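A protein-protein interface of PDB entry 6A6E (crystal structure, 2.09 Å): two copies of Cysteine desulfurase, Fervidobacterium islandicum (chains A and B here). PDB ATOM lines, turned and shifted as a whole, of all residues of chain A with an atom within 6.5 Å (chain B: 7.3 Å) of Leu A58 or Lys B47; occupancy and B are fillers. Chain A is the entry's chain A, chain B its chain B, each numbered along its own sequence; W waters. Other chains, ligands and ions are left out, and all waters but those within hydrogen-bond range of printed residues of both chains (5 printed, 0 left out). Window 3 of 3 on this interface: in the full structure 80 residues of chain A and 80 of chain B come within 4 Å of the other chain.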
ATOM      1  N   MET A  53      20.042  22.243  28.850  1.00  0.00           N
ATOM      2  CA  MET A  53      20.290  23.194  27.748  1.00  0.00           C
ATOM      3  C   MET A  53      19.240  23.196  26.685  1.00  0.00           C
ATOM      4  O   MET A  53      18.841  24.274  26.172  1.00  0.00           O
ATOM      5  CB  MET A  53      21.608  22.884  27.068  1.00  0.00           C
ATOM      6  CG  MET A  53      22.809  23.074  27.988  1.00  0.00           C
ATOM      7  SD  MET A  53      24.378  22.516  27.222  1.00  0.00           S
ATOM      8  CE  MET A  53      24.322  23.471  25.748  1.00  0.00           C
ATOM      9  N   THR A  54      18.762  22.005  26.360  1.00  0.00           N
ATOM     10  CA  THR A  54      17.659  21.833  25.426  1.00  0.00           C
ATOM     11  C   THR A  54      16.352  22.526  25.911  1.00  0.00           C
ATOM     12  O   THR A  54      15.715  23.255  25.167  1.00  0.00           O
ATOM     13  CB  THR A  54      17.335  20.333  25.219  1.00  0.00           C
ATOM     14  OG1 THR A  54      18.369  19.723  24.469  1.00  0.00           O
ATOM     15  CG2 THR A  54      16.019  20.171  24.411  1.00  0.00           C
ATOM     16  N   ASP A  55      15.995  22.319  27.173  1.00  0.00           N
ATOM     17  CA  ASP A  55      14.859  22.993  27.787  1.00  0.00           C
ATOM     18  C   ASP A  55      15.028  24.541  27.753  1.00  0.00           C
ATOM     19  O   ASP A  55      14.093  25.278  27.474  1.00  0.00           O
ATOM     20  CB  ASP A  55      14.664  22.496  29.230  1.00  0.00           C
ATOM     21  CG  ASP A  55      13.663  23.354  30.031  1.00  0.00           C
ATOM     22  OD1 ASP A  55      12.459  23.139  29.867  1.00  0.00           O
ATOM     23  OD2 ASP A  55      14.085  24.275  30.800  1.00  0.00           O
ATOM     24  N   PHE A  56      16.251  25.004  28.013  1.00  0.00           N
ATOM     25  CA  PHE A  56      16.535  26.395  27.932  1.00  0.00           C
ATOM     26  C   PHE A  56      16.336  26.956  26.495  1.00  0.00           C
ATOM     27  O   PHE A  56      15.596  27.915  26.320  1.00  0.00           O
ATOM     28  CB  PHE A  56      17.942  26.696  28.461  1.00  0.00           C
ATOM     29  CG  PHE A  56      18.262  28.160  28.437  1.00  0.00           C
ATOM     30  CD1 PHE A  56      17.787  29.000  29.443  1.00  0.00           C
ATOM     31  CD2 PHE A  56      18.980  28.712  27.385  1.00  0.00           C
ATOM     32  CE1 PHE A  56      18.056  30.391  29.408  1.00  0.00           C
ATOM     33  CE2 PHE A  56      19.263  30.071  27.345  1.00  0.00           C
ATOM     34  CZ  PHE A  56      18.796  30.904  28.380  1.00  0.00           C
ATOM     35  N   TYR A  57      16.927  26.311  25.482  1.00  0.00           N
ATOM     36  CA  TYR A  57      16.771  26.714  24.082  1.00  0.00           C
ATOM     37  C   TYR A  57      15.325  26.735  23.655  1.00  0.00           C
ATOM     38  O   TYR A  57      14.913  27.598  22.835  1.00  0.00           O
ATOM     39  CB  TYR A  57      17.530  25.761  23.120  1.00  0.00           C
ATOM     40  CG  TYR A  57      18.965  26.124  22.693  1.00  0.00           C
ATOM     41  CD1 TYR A  57      19.299  27.412  22.244  1.00  0.00           C
ATOM     42  CD2 TYR A  57      19.979  25.150  22.657  1.00  0.00           C
ATOM     43  CE1 TYR A  57      20.588  27.716  21.834  1.00  0.00           C
ATOM     44  CE2 TYR A  57      21.265  25.449  22.222  1.00  0.00           C
ATOM     45  CZ  TYR A  57      21.540  26.751  21.789  1.00  0.00           C
ATOM     46  OH  TYR A  57      22.792  27.064  21.396  1.00  0.00           O
ATOM     47  N   LEU A  58      14.550  25.737  24.126  1.00  0.00           N
ATOM     48  CA  LEU A  58      13.207  25.538  23.558  1.00  0.00           C
ATOM     49  C   LEU A  58      12.159  26.368  24.320  1.00  0.00           C
ATOM     50  O   LEU A  58      11.184  26.751  23.733  1.00  0.00           O
ATOM     51  CB  LEU A  58      12.811  24.051  23.513  1.00  0.00           C
ATOM     52  CG  LEU A  58      13.606  23.179  22.542  1.00  0.00           C
ATOM     53  CD1 LEU A  58      13.248  21.704  22.674  1.00  0.00           C
ATOM     54  CD2 LEU A  58      13.419  23.686  21.093  1.00  0.00           C
ATOM     55  N   TYR A  59      12.372  26.661  25.596  1.00  0.00           N
ATOM     56  CA  TYR A  59      11.323  27.285  26.416  1.00  0.00           C
ATOM     57  C   TYR A  59      11.711  28.588  27.140  1.00  0.00           C
ATOM     58  O   TYR A  59      10.798  29.339  27.587  1.00  0.00           O
ATOM     59  CB  TYR A  59      10.761  26.266  27.443  1.00  0.00           C
ATOM     60  CG  TYR A  59      10.030  25.047  26.823  1.00  0.00           C
ATOM     61  CD1 TYR A  59       8.731  25.168  26.295  1.00  0.00           C
ATOM     62  CD2 TYR A  59      10.635  23.823  26.738  1.00  0.00           C
ATOM     63  CE1 TYR A  59       8.051  24.063  25.715  1.00  0.00           C
ATOM     64  CE2 TYR A  59       9.954  22.699  26.204  1.00  0.00           C
ATOM     65  CZ  TYR A  59       8.660  22.841  25.691  1.00  0.00           C
ATOM     66  OH  TYR A  59       8.002  21.772  25.130  1.00  0.00           O
ATOM     67  N   HIS A  60      13.003  28.881  27.270  1.00  0.00           N
ATOM     68  CA  HIS A  60      13.414  30.021  28.110  1.00  0.00           C
ATOM     69  C   HIS A  60      14.352  30.994  27.407  1.00  0.00           C
ATOM     70  O   HIS A  60      15.102  31.664  28.034  1.00  0.00           O
ATOM     71  CB  HIS A  60      14.016  29.551  29.398  1.00  0.00           C
ATOM     72  CG  HIS A  60      13.067  28.696  30.185  1.00  0.00           C
ATOM     73  ND1 HIS A  60      11.973  29.222  30.837  1.00  0.00           N
ATOM     74  CD2 HIS A  60      12.971  27.346  30.306  1.00  0.00           C
ATOM     75  CE1 HIS A  60      11.281  28.233  31.375  1.00  0.00           C
ATOM     76  NE2 HIS A  60      11.855  27.083  31.060  1.00  0.00           N
ATOM     77  N   TYR A  61      14.261  31.058  26.099  1.00  0.00           N
ATOM     78  CA  TYR A  61      15.344  31.653  25.292  1.00  0.00           C
ATOM     79  C   TYR A  61      14.925  32.946  24.627  1.00  0.00           C
ATOM     80  O   TYR A  61      13.847  33.025  24.081  1.00  0.00           O
ATOM     81  CB  TYR A  61      15.790  30.662  24.211  1.00  0.00           C
ATOM     82  CG  TYR A  61      16.782  31.311  23.293  1.00  0.00           C
ATOM     83  CD1 TYR A  61      18.119  31.358  23.644  1.00  0.00           C
ATOM     84  CD2 TYR A  61      16.377  32.014  22.169  1.00  0.00           C
ATOM     85  CE1 TYR A  61      19.030  32.008  22.846  1.00  0.00           C
ATOM     86  CE2 TYR A  61      17.281  32.674  21.383  1.00  0.00           C
ATOM     87  CZ  TYR A  61      18.612  32.643  21.731  1.00  0.00           C
ATOM     88  OH  TYR A  61      19.566  33.294  20.989  1.00  0.00           O
ATOM     89  N   ASN B  20       4.283  24.049  14.831  1.00  0.00           N
ATOM     90  CA  ASN B  20       4.515  23.008  15.823  1.00  0.00           C
ATOM     91  C   ASN B  20       6.005  22.707  16.078  1.00  0.00           C
ATOM     92  O   ASN B  20       6.313  22.074  17.051  1.00  0.00           O
ATOM     93  CB  ASN B  20       3.766  21.703  15.461  1.00  0.00           C
ATOM     94  CG  ASN B  20       2.295  21.708  15.930  1.00  0.00           C
ATOM     95  OD1 ASN B  20       1.853  22.580  16.697  1.00  0.00           O
ATOM     96  ND2 ASN B  20       1.515  20.770  15.405  1.00  0.00           N
ATOM     97  N   ASP B  21       6.901  23.138  15.200  1.00  0.00           N
ATOM     98  CA  ASP B  21       8.365  22.939  15.399  1.00  0.00           C
ATOM     99  C   ASP B  21       8.937  23.776  16.493  1.00  0.00           C
ATOM    100  O   ASP B  21      10.066  23.506  16.959  1.00  0.00           O
ATOM    101  CB  ASP B  21       9.119  23.237  14.117  1.00  0.00           C
ATOM    102  CG  ASP B  21       8.822  22.189  12.986  1.00  0.00           C
ATOM    103  OD1 ASP B  21       8.767  21.015  13.308  1.00  0.00           O
ATOM    104  OD2 ASP B  21       8.652  22.543  11.790  1.00  0.00           O
ATOM    105  N   PHE B  22       8.172  24.745  16.995  1.00  0.00           N
ATOM    106  CA  PHE B  22       8.739  25.747  17.942  1.00  0.00           C
ATOM    107  C   PHE B  22       7.993  25.709  19.259  1.00  0.00           C
ATOM    108  O   PHE B  22       6.981  26.380  19.403  1.00  0.00           O
ATOM    109  CB  PHE B  22       8.642  27.151  17.306  1.00  0.00           C
ATOM    110  CG  PHE B  22       9.444  27.270  16.063  1.00  0.00           C
ATOM    111  CD1 PHE B  22      10.816  27.545  16.113  1.00  0.00           C
ATOM    112  CD2 PHE B  22       8.873  26.988  14.829  1.00  0.00           C
ATOM    113  CE1 PHE B  22      11.579  27.580  14.935  1.00  0.00           C
ATOM    114  CE2 PHE B  22       9.622  27.044  13.669  1.00  0.00           C
ATOM    115  CZ  PHE B  22      10.966  27.311  13.716  1.00  0.00           C
ATOM    116  N   PRO B  23       8.493  24.948  20.228  1.00  0.00           N
ATOM    117  CA  PRO B  23       7.702  24.742  21.434  1.00  0.00           C
ATOM    118  C   PRO B  23       7.502  26.002  22.260  1.00  0.00           C
ATOM    119  O   PRO B  23       6.543  26.065  23.027  1.00  0.00           O
ATOM    120  CB  PRO B  23       8.495  23.692  22.226  1.00  0.00           C
ATOM    121  CG  PRO B  23       9.367  22.988  21.206  1.00  0.00           C
ATOM    122  CD  PRO B  23       9.611  23.987  20.118  1.00  0.00           C
ATOM    123  N   ALA B  24       8.311  27.039  22.066  1.00  0.00           N
ATOM    124  CA  ALA B  24       8.136  28.255  22.853  1.00  0.00           C
ATOM    125  C   ALA B  24       6.738  28.858  22.620  1.00  0.00           C
ATOM    126  O   ALA B  24       6.177  29.517  23.476  1.00  0.00           O
ATOM    127  CB  ALA B  24       9.223  29.265  22.547  1.00  0.00           C
ATOM    128  N   LEU B  25       6.199  28.643  21.436  1.00  0.00           N
ATOM    129  CA  LEU B  25       4.925  29.148  21.086  1.00  0.00           C
ATOM    130  C   LEU B  25       3.753  28.586  21.952  1.00  0.00           C
ATOM    131  O   LEU B  25       2.693  29.212  22.004  1.00  0.00           O
ATOM    132  CB  LEU B  25       4.683  28.944  19.624  1.00  0.00           C
ATOM    133  CG  LEU B  25       5.669  29.573  18.640  1.00  0.00           C
ATOM    134  CD1 LEU B  25       5.208  29.220  17.235  1.00  0.00           C
ATOM    135  CD2 LEU B  25       5.817  31.056  18.780  1.00  0.00           C
ATOM    136  N   ARG B  27       3.971  28.694  25.189  1.00  0.00           N
ATOM    137  CA  ARG B  27       4.058  29.349  26.463  1.00  0.00           C
ATOM    138  C   ARG B  27       2.883  30.335  26.541  1.00  0.00           C
ATOM    139  O   ARG B  27       2.434  30.858  25.519  1.00  0.00           O
ATOM    140  CB  ARG B  27       5.357  30.147  26.620  1.00  0.00           C
ATOM    141  CG  ARG B  27       6.656  29.369  26.793  1.00  0.00           C
ATOM    142  CD  ARG B  27       7.056  28.966  28.181  1.00  0.00           C
ATOM    143  NE  ARG B  27       6.830  30.010  29.175  1.00  0.00           N
ATOM    144  CZ  ARG B  27       7.764  30.779  29.695  1.00  0.00           C
ATOM    145  NH1 ARG B  27       9.035  30.626  29.343  1.00  0.00           N
ATOM    146  NH2 ARG B  27       7.421  31.723  30.593  1.00  0.00           N
ATOM    147  N   LEU B  44      13.503  32.215  17.966  1.00  0.00           N
ATOM    148  CA  LEU B  44      13.130  30.939  18.606  1.00  0.00           C
ATOM    149  C   LEU B  44      13.793  29.712  17.903  1.00  0.00           C
ATOM    150  O   LEU B  44      14.200  29.771  16.717  1.00  0.00           O
ATOM    151  CB  LEU B  44      11.644  30.765  18.646  1.00  0.00           C
ATOM    152  CG  LEU B  44      10.807  31.941  19.188  1.00  0.00           C
ATOM    153  CD1 LEU B  44       9.306  31.692  19.030  1.00  0.00           C
ATOM    154  CD2 LEU B  44      11.236  32.244  20.615  1.00  0.00           C
ATOM    155  N   LYS B  45      13.876  28.581  18.632  1.00  0.00           N
ATOM    156  CA  LYS B  45      14.575  27.363  18.169  1.00  0.00           C
ATOM    157  C   LYS B  45      13.577  26.230  17.843  1.00  0.00           C
ATOM    158  O   LYS B  45      12.532  26.063  18.505  1.00  0.00           O
ATOM    159  CB  LYS B  45      15.555  26.868  19.253  1.00  0.00           C
ATOM    160  CG  LYS B  45      16.441  27.943  19.825  1.00  0.00           C
ATOM    161  CD  LYS B  45      17.116  28.789  18.760  1.00  0.00           C
ATOM    162  CE  LYS B  45      17.923  29.914  19.406  1.00  0.00           C
ATOM    163  NZ  LYS B  45      18.219  30.967  18.390  1.00  0.00           N
ATOM    164  N   CYS B  46      13.921  25.513  16.777  1.00  0.00           N
ATOM    165  CA  CYS B  46      13.194  24.406  16.223  1.00  0.00           C
ATOM    166  C   CYS B  46      13.549  23.148  17.011  1.00  0.00           C
ATOM    167  O   CYS B  46      14.733  22.839  17.186  1.00  0.00           O
ATOM    168  CB  CYS B  46      13.704  24.202  14.770  1.00  0.00           C
ATOM    169  SG  CYS B  46      12.901  22.841  14.026  1.00  0.00           S
ATOM    170  N   LYS B  47      12.556  22.381  17.414  1.00  0.00           N
ATOM    171  CA  LYS B  47      12.800  21.196  18.238  1.00  0.00           C
ATOM    172  C   LYS B  47      13.609  20.112  17.479  1.00  0.00           C
ATOM    173  O   LYS B  47      14.523  19.524  18.030  1.00  0.00           O
ATOM    174  CB  LYS B  47      11.475  20.593  18.717  1.00  0.00           C
ATOM    175  CG  LYS B  47      11.665  19.391  19.588  1.00  0.00           C
ATOM    176  CD  LYS B  47      10.345  19.006  20.205  1.00  0.00           C
ATOM    177  CE  LYS B  47      10.600  18.010  21.298  1.00  0.00           C
ATOM    178  NZ  LYS B  47       9.333  17.259  21.424  1.00  0.00           N
ATOM    179  N   SER B  48      13.297  19.871  16.223  1.00  0.00           N
ATOM    180  CA  SER B  48      14.007  18.813  15.491  1.00  0.00           C
ATOM    181  C   SER B  48      15.472  19.158  15.311  1.00  0.00           C
ATOM    182  O   SER B  48      16.363  18.254  15.319  1.00  0.00           O
ATOM    183  CB  SER B  48      13.355  18.486  14.138  1.00  0.00           C
ATOM    184  OG  SER B  48      13.272  19.614  13.271  1.00  0.00           O
ATOM    185  N   VAL B  49      15.741  20.463  15.174  1.00  0.00           N
ATOM    186  CA  VAL B  49      17.111  20.913  15.062  1.00  0.00           C
ATOM    187  C   VAL B  49      17.883  20.688  16.350  1.00  0.00           C
ATOM    188  O   VAL B  49      19.017  20.199  16.326  1.00  0.00           O
ATOM    189  CB  VAL B  49      17.189  22.390  14.577  1.00  0.00           C
ATOM    190  CG1 VAL B  49      18.626  22.909  14.566  1.00  0.00           C
ATOM    191  CG2 VAL B  49      16.634  22.464  13.162  1.00  0.00           C
ATOM    192  N   ILE B  50      17.305  21.128  17.462  1.00  0.00           N
ATOM    193  CA  ILE B  50      17.941  20.981  18.734  1.00  0.00           C
ATOM    194  C   ILE B  50      18.114  19.484  19.113  1.00  0.00           C
ATOM    195  O   ILE B  50      19.115  19.114  19.741  1.00  0.00           O
ATOM    196  CB  ILE B  50      17.153  21.684  19.855  1.00  0.00           C
ATOM    197  CG1 ILE B  50      16.961  23.200  19.573  1.00  0.00           C
ATOM    198  CG2 ILE B  50      17.874  21.517  21.159  1.00  0.00           C
ATOM    199  CD1 ILE B  50      18.236  23.976  19.396  1.00  0.00           C
ATOM    200  N   GLU B  51      17.154  18.635  18.748  1.00  0.00           N
ATOM    201  CA  GLU B  51      17.320  17.153  18.918  1.00  0.00           C
ATOM    202  C   GLU B  51      18.555  16.585  18.149  1.00  0.00           C
ATOM    203  O   GLU B  51      19.265  15.727  18.632  1.00  0.00           O
ATOM    204  CB  GLU B  51      15.998  16.400  18.498  1.00  0.00           C
ATOM    205  CG  GLU B  51      14.793  16.693  19.430  1.00  0.00           C
ATOM    206  CD  GLU B  51      13.434  16.010  19.024  1.00  0.00           C
ATOM    207  OE1 GLU B  51      13.127  15.767  17.819  1.00  0.00           O
ATOM    208  OE2 GLU B  51      12.627  15.722  19.934  1.00  0.00           O
ATOM    209  N   LYS B  52      18.797  17.071  16.950  1.00  0.00           N
ATOM    210  CA  LYS B  52      19.995  16.686  16.208  1.00  0.00           C
ATOM    211  C   LYS B  52      21.262  17.131  16.858  1.00  0.00           C
ATOM    212  O   LYS B  52      22.249  16.401  16.887  1.00  0.00           O
ATOM    213  CB  LYS B  52      19.942  17.206  14.774  1.00  0.00           C
ATOM    214  CG  LYS B  52      18.911  16.427  13.981  1.00  0.00           C
ATOM    215  CD  LYS B  52      18.850  16.935  12.560  1.00  0.00           C
ATOM    216  CE  LYS B  52      17.762  16.197  11.822  1.00  0.00           C
ATOM    217  NZ  LYS B  52      17.721  16.720  10.441  1.00  0.00           N
ATOM    218  N   MET B  53      21.252  18.342  17.391  1.00  0.00           N
ATOM    219  CA  MET B  53      22.404  18.804  18.171  1.00  0.00           C
ATOM    220  C   MET B  53      22.649  17.990  19.409  1.00  0.00           C
ATOM    221  O   MET B  53      23.807  17.694  19.763  1.00  0.00           O
ATOM    222  CB  MET B  53      22.222  20.246  18.601  1.00  0.00           C
ATOM    223  CG  MET B  53      22.214  21.196  17.432  1.00  0.00           C
ATOM    224  SD  MET B  53      21.799  22.858  17.966  1.00  0.00           S
ATOM    225  CE  MET B  53      23.195  23.205  18.993  1.00  0.00           C
ATOM    226  N   THR B  54      21.558  17.647  20.080  1.00  0.00           N
ATOM    227  CA  THR B  54      21.604  16.755  21.227  1.00  0.00           C
ATOM    228  C   THR B  54      22.227  15.360  20.848  1.00  0.00           C
ATOM    229  O   THR B  54      23.130  14.862  21.520  1.00  0.00           O
ATOM    230  CB  THR B  54      20.184  16.619  21.824  1.00  0.00           C
ATOM    231  OG1 THR B  54      19.836  17.864  22.437  1.00  0.00           O
ATOM    232  CG2 THR B  54      20.105  15.494  22.828  1.00  0.00           C
ATOM    233  N   TYR B 302      16.919  22.566   7.624  1.00  0.00           N
ATOM    234  CA  TYR B 302      15.516  22.778   7.983  1.00  0.00           C
ATOM    235  C   TYR B 302      14.877  23.861   7.139  1.00  0.00           C
ATOM    236  O   TYR B 302      13.799  23.660   6.536  1.00  0.00           O
ATOM    237  CB  TYR B 302      15.368  23.047   9.495  1.00  0.00           C
ATOM    238  CG  TYR B 302      14.008  23.450   9.927  1.00  0.00           C
ATOM    239  CD1 TYR B 302      12.968  22.502  10.061  1.00  0.00           C
ATOM    240  CD2 TYR B 302      13.688  24.780  10.152  1.00  0.00           C
ATOM    241  CE1 TYR B 302      11.660  22.893  10.451  1.00  0.00           C
ATOM    242  CE2 TYR B 302      12.381  25.187  10.533  1.00  0.00           C
ATOM    243  CZ  TYR B 302      11.370  24.216  10.703  1.00  0.00           C
ATOM    244  OH  TYR B 302      10.072  24.603  11.040  1.00  0.00           O
HETATM  245  O   HOH W   1      20.793  20.750  23.421  1.00  0.00           O
HETATM  246  O   HOH W   2      17.128  17.580  22.441  1.00  0.00           O
HETATM  247  O   HOH W   3      12.951  28.859  21.528  1.00  0.00           O
HETATM  248  O   HOH W   4      10.917  27.217  20.452  1.00  0.00           O
HETATM  249  O   HOH W   5      18.419  17.192  25.037  1.00  0.00           O
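O of Tyr A59 lies within hydrogen-bond range of NH1 of Arg B27 (2.8 Å).
OG1 of Thr B54 lies within hydrogen-bond range of OG1 of Thr A54.
The backbone carbonyl oxygen of Leu A58 sits at hydrogen-bond distance from the backbone NH of Ala B24, 3.3 Å away.
The backbone carbonyl oxygen (O) of Phe A56 lies within hydrogen-bond range of the backbone NH (N) of Tyr A61 (3.4 Å).
NZ of Lys B47 lies within salt-bridge range of OE2 of Glu B51, at 3.9 Å.
The backbone carbonyl oxygen (O) of Asp B21 sits at hydrogen-bond distance from the backbone NH (N) of Lys B47 (2.8 Å).
OG1 of Thr B54 lies within hydrogen-bond range of O of Ile B50, at 3.1 Å.
Among the printed residues, pairs that only touch across the chains: Thr A54 with Ile B50, Tyr A57 with Lys B45, Tyr A57 with Ile B50, Leu A58 with Pro B23, Leu A58 with Lys B45, Leu A58 with Lys B47, Leu A58 with Ile B50, Tyr A59 with Pro B23, His A60 with Arg B27 and Tyr A61 with Lys B45.
Of the printed residues of chain B, Thr A54 touches Ile B50 and Thr B54.
Printed residues of chain B within 4 Å of Tyr A57: Lys B45 (3.4 Å) and Ile B50 (3.9 Å).
Of chain B, only Pro B23, Ala B24, Lys B45, Lys B47 and Ile B50 come within 4 Å of Leu A58.
Of the printed residues of chain A, Arg B27 touches Tyr A59 and His A60.
Lys B47 touches just one residue of chain A: Leu A58.
The nearest residue of chain B that does not touch Leu A58 is Cys B46 (4.1 Å).
The nearest residue of chain A that does not touch Lys B47 is Tyr A59 (6.0 Å).
Of the 19 printed residues of chain B, 7 touch a printed residue of chain A.
Hydrophobic or aromatic side chains of chain B within 4 Å of the printed part of chain A: Pro B23, Ala B24 and Ile B50.
Of the 9 printed residues of chain A, 6 touch a printed residue of chain B.
Printed residues of chain A that touch a printed residue of chain B: Thr A54, Tyr A57, Leu A58, Tyr A59, His A60 and Tyr A61.
Along chain A the printed residues that touch a printed residue of chain B span positions 54 to 61.
Among the printed residues, 13 pairs touch across the chains.
Thr A54 touches its own counterpart, Thr B54.
2 positions are printed for both chains.
Of the 13 pairs that touch across the chains among the printed residues, 1 has its exchanged pair printed and touching as well.
Water W5 lies within hydrogen-bond range of OG1 of Thr A54 (2.6 Å) and OG1 of Thr B54 (3.0 Å).
Water W3 lies within hydrogen-bond range of the backbone carbonyl oxygen (O) of Tyr A57 (2.7 Å) and the backbone NH (N) of Lys B45 (3.1 Å).
Water W2 bridges OG1 of Thr B54 and OG1 of Thr A54.
Water W4 lies within hydrogen-bond range of O of Lys B45 (2.8 Å), N of Ala B24 (3.1 Å) and O of Leu A58 (3.3 Å).
Water W1 lies within hydrogen-bond range of OG1 of Thr A54 (2.8 Å) and OG1 of Thr B54 (3.2 Å).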
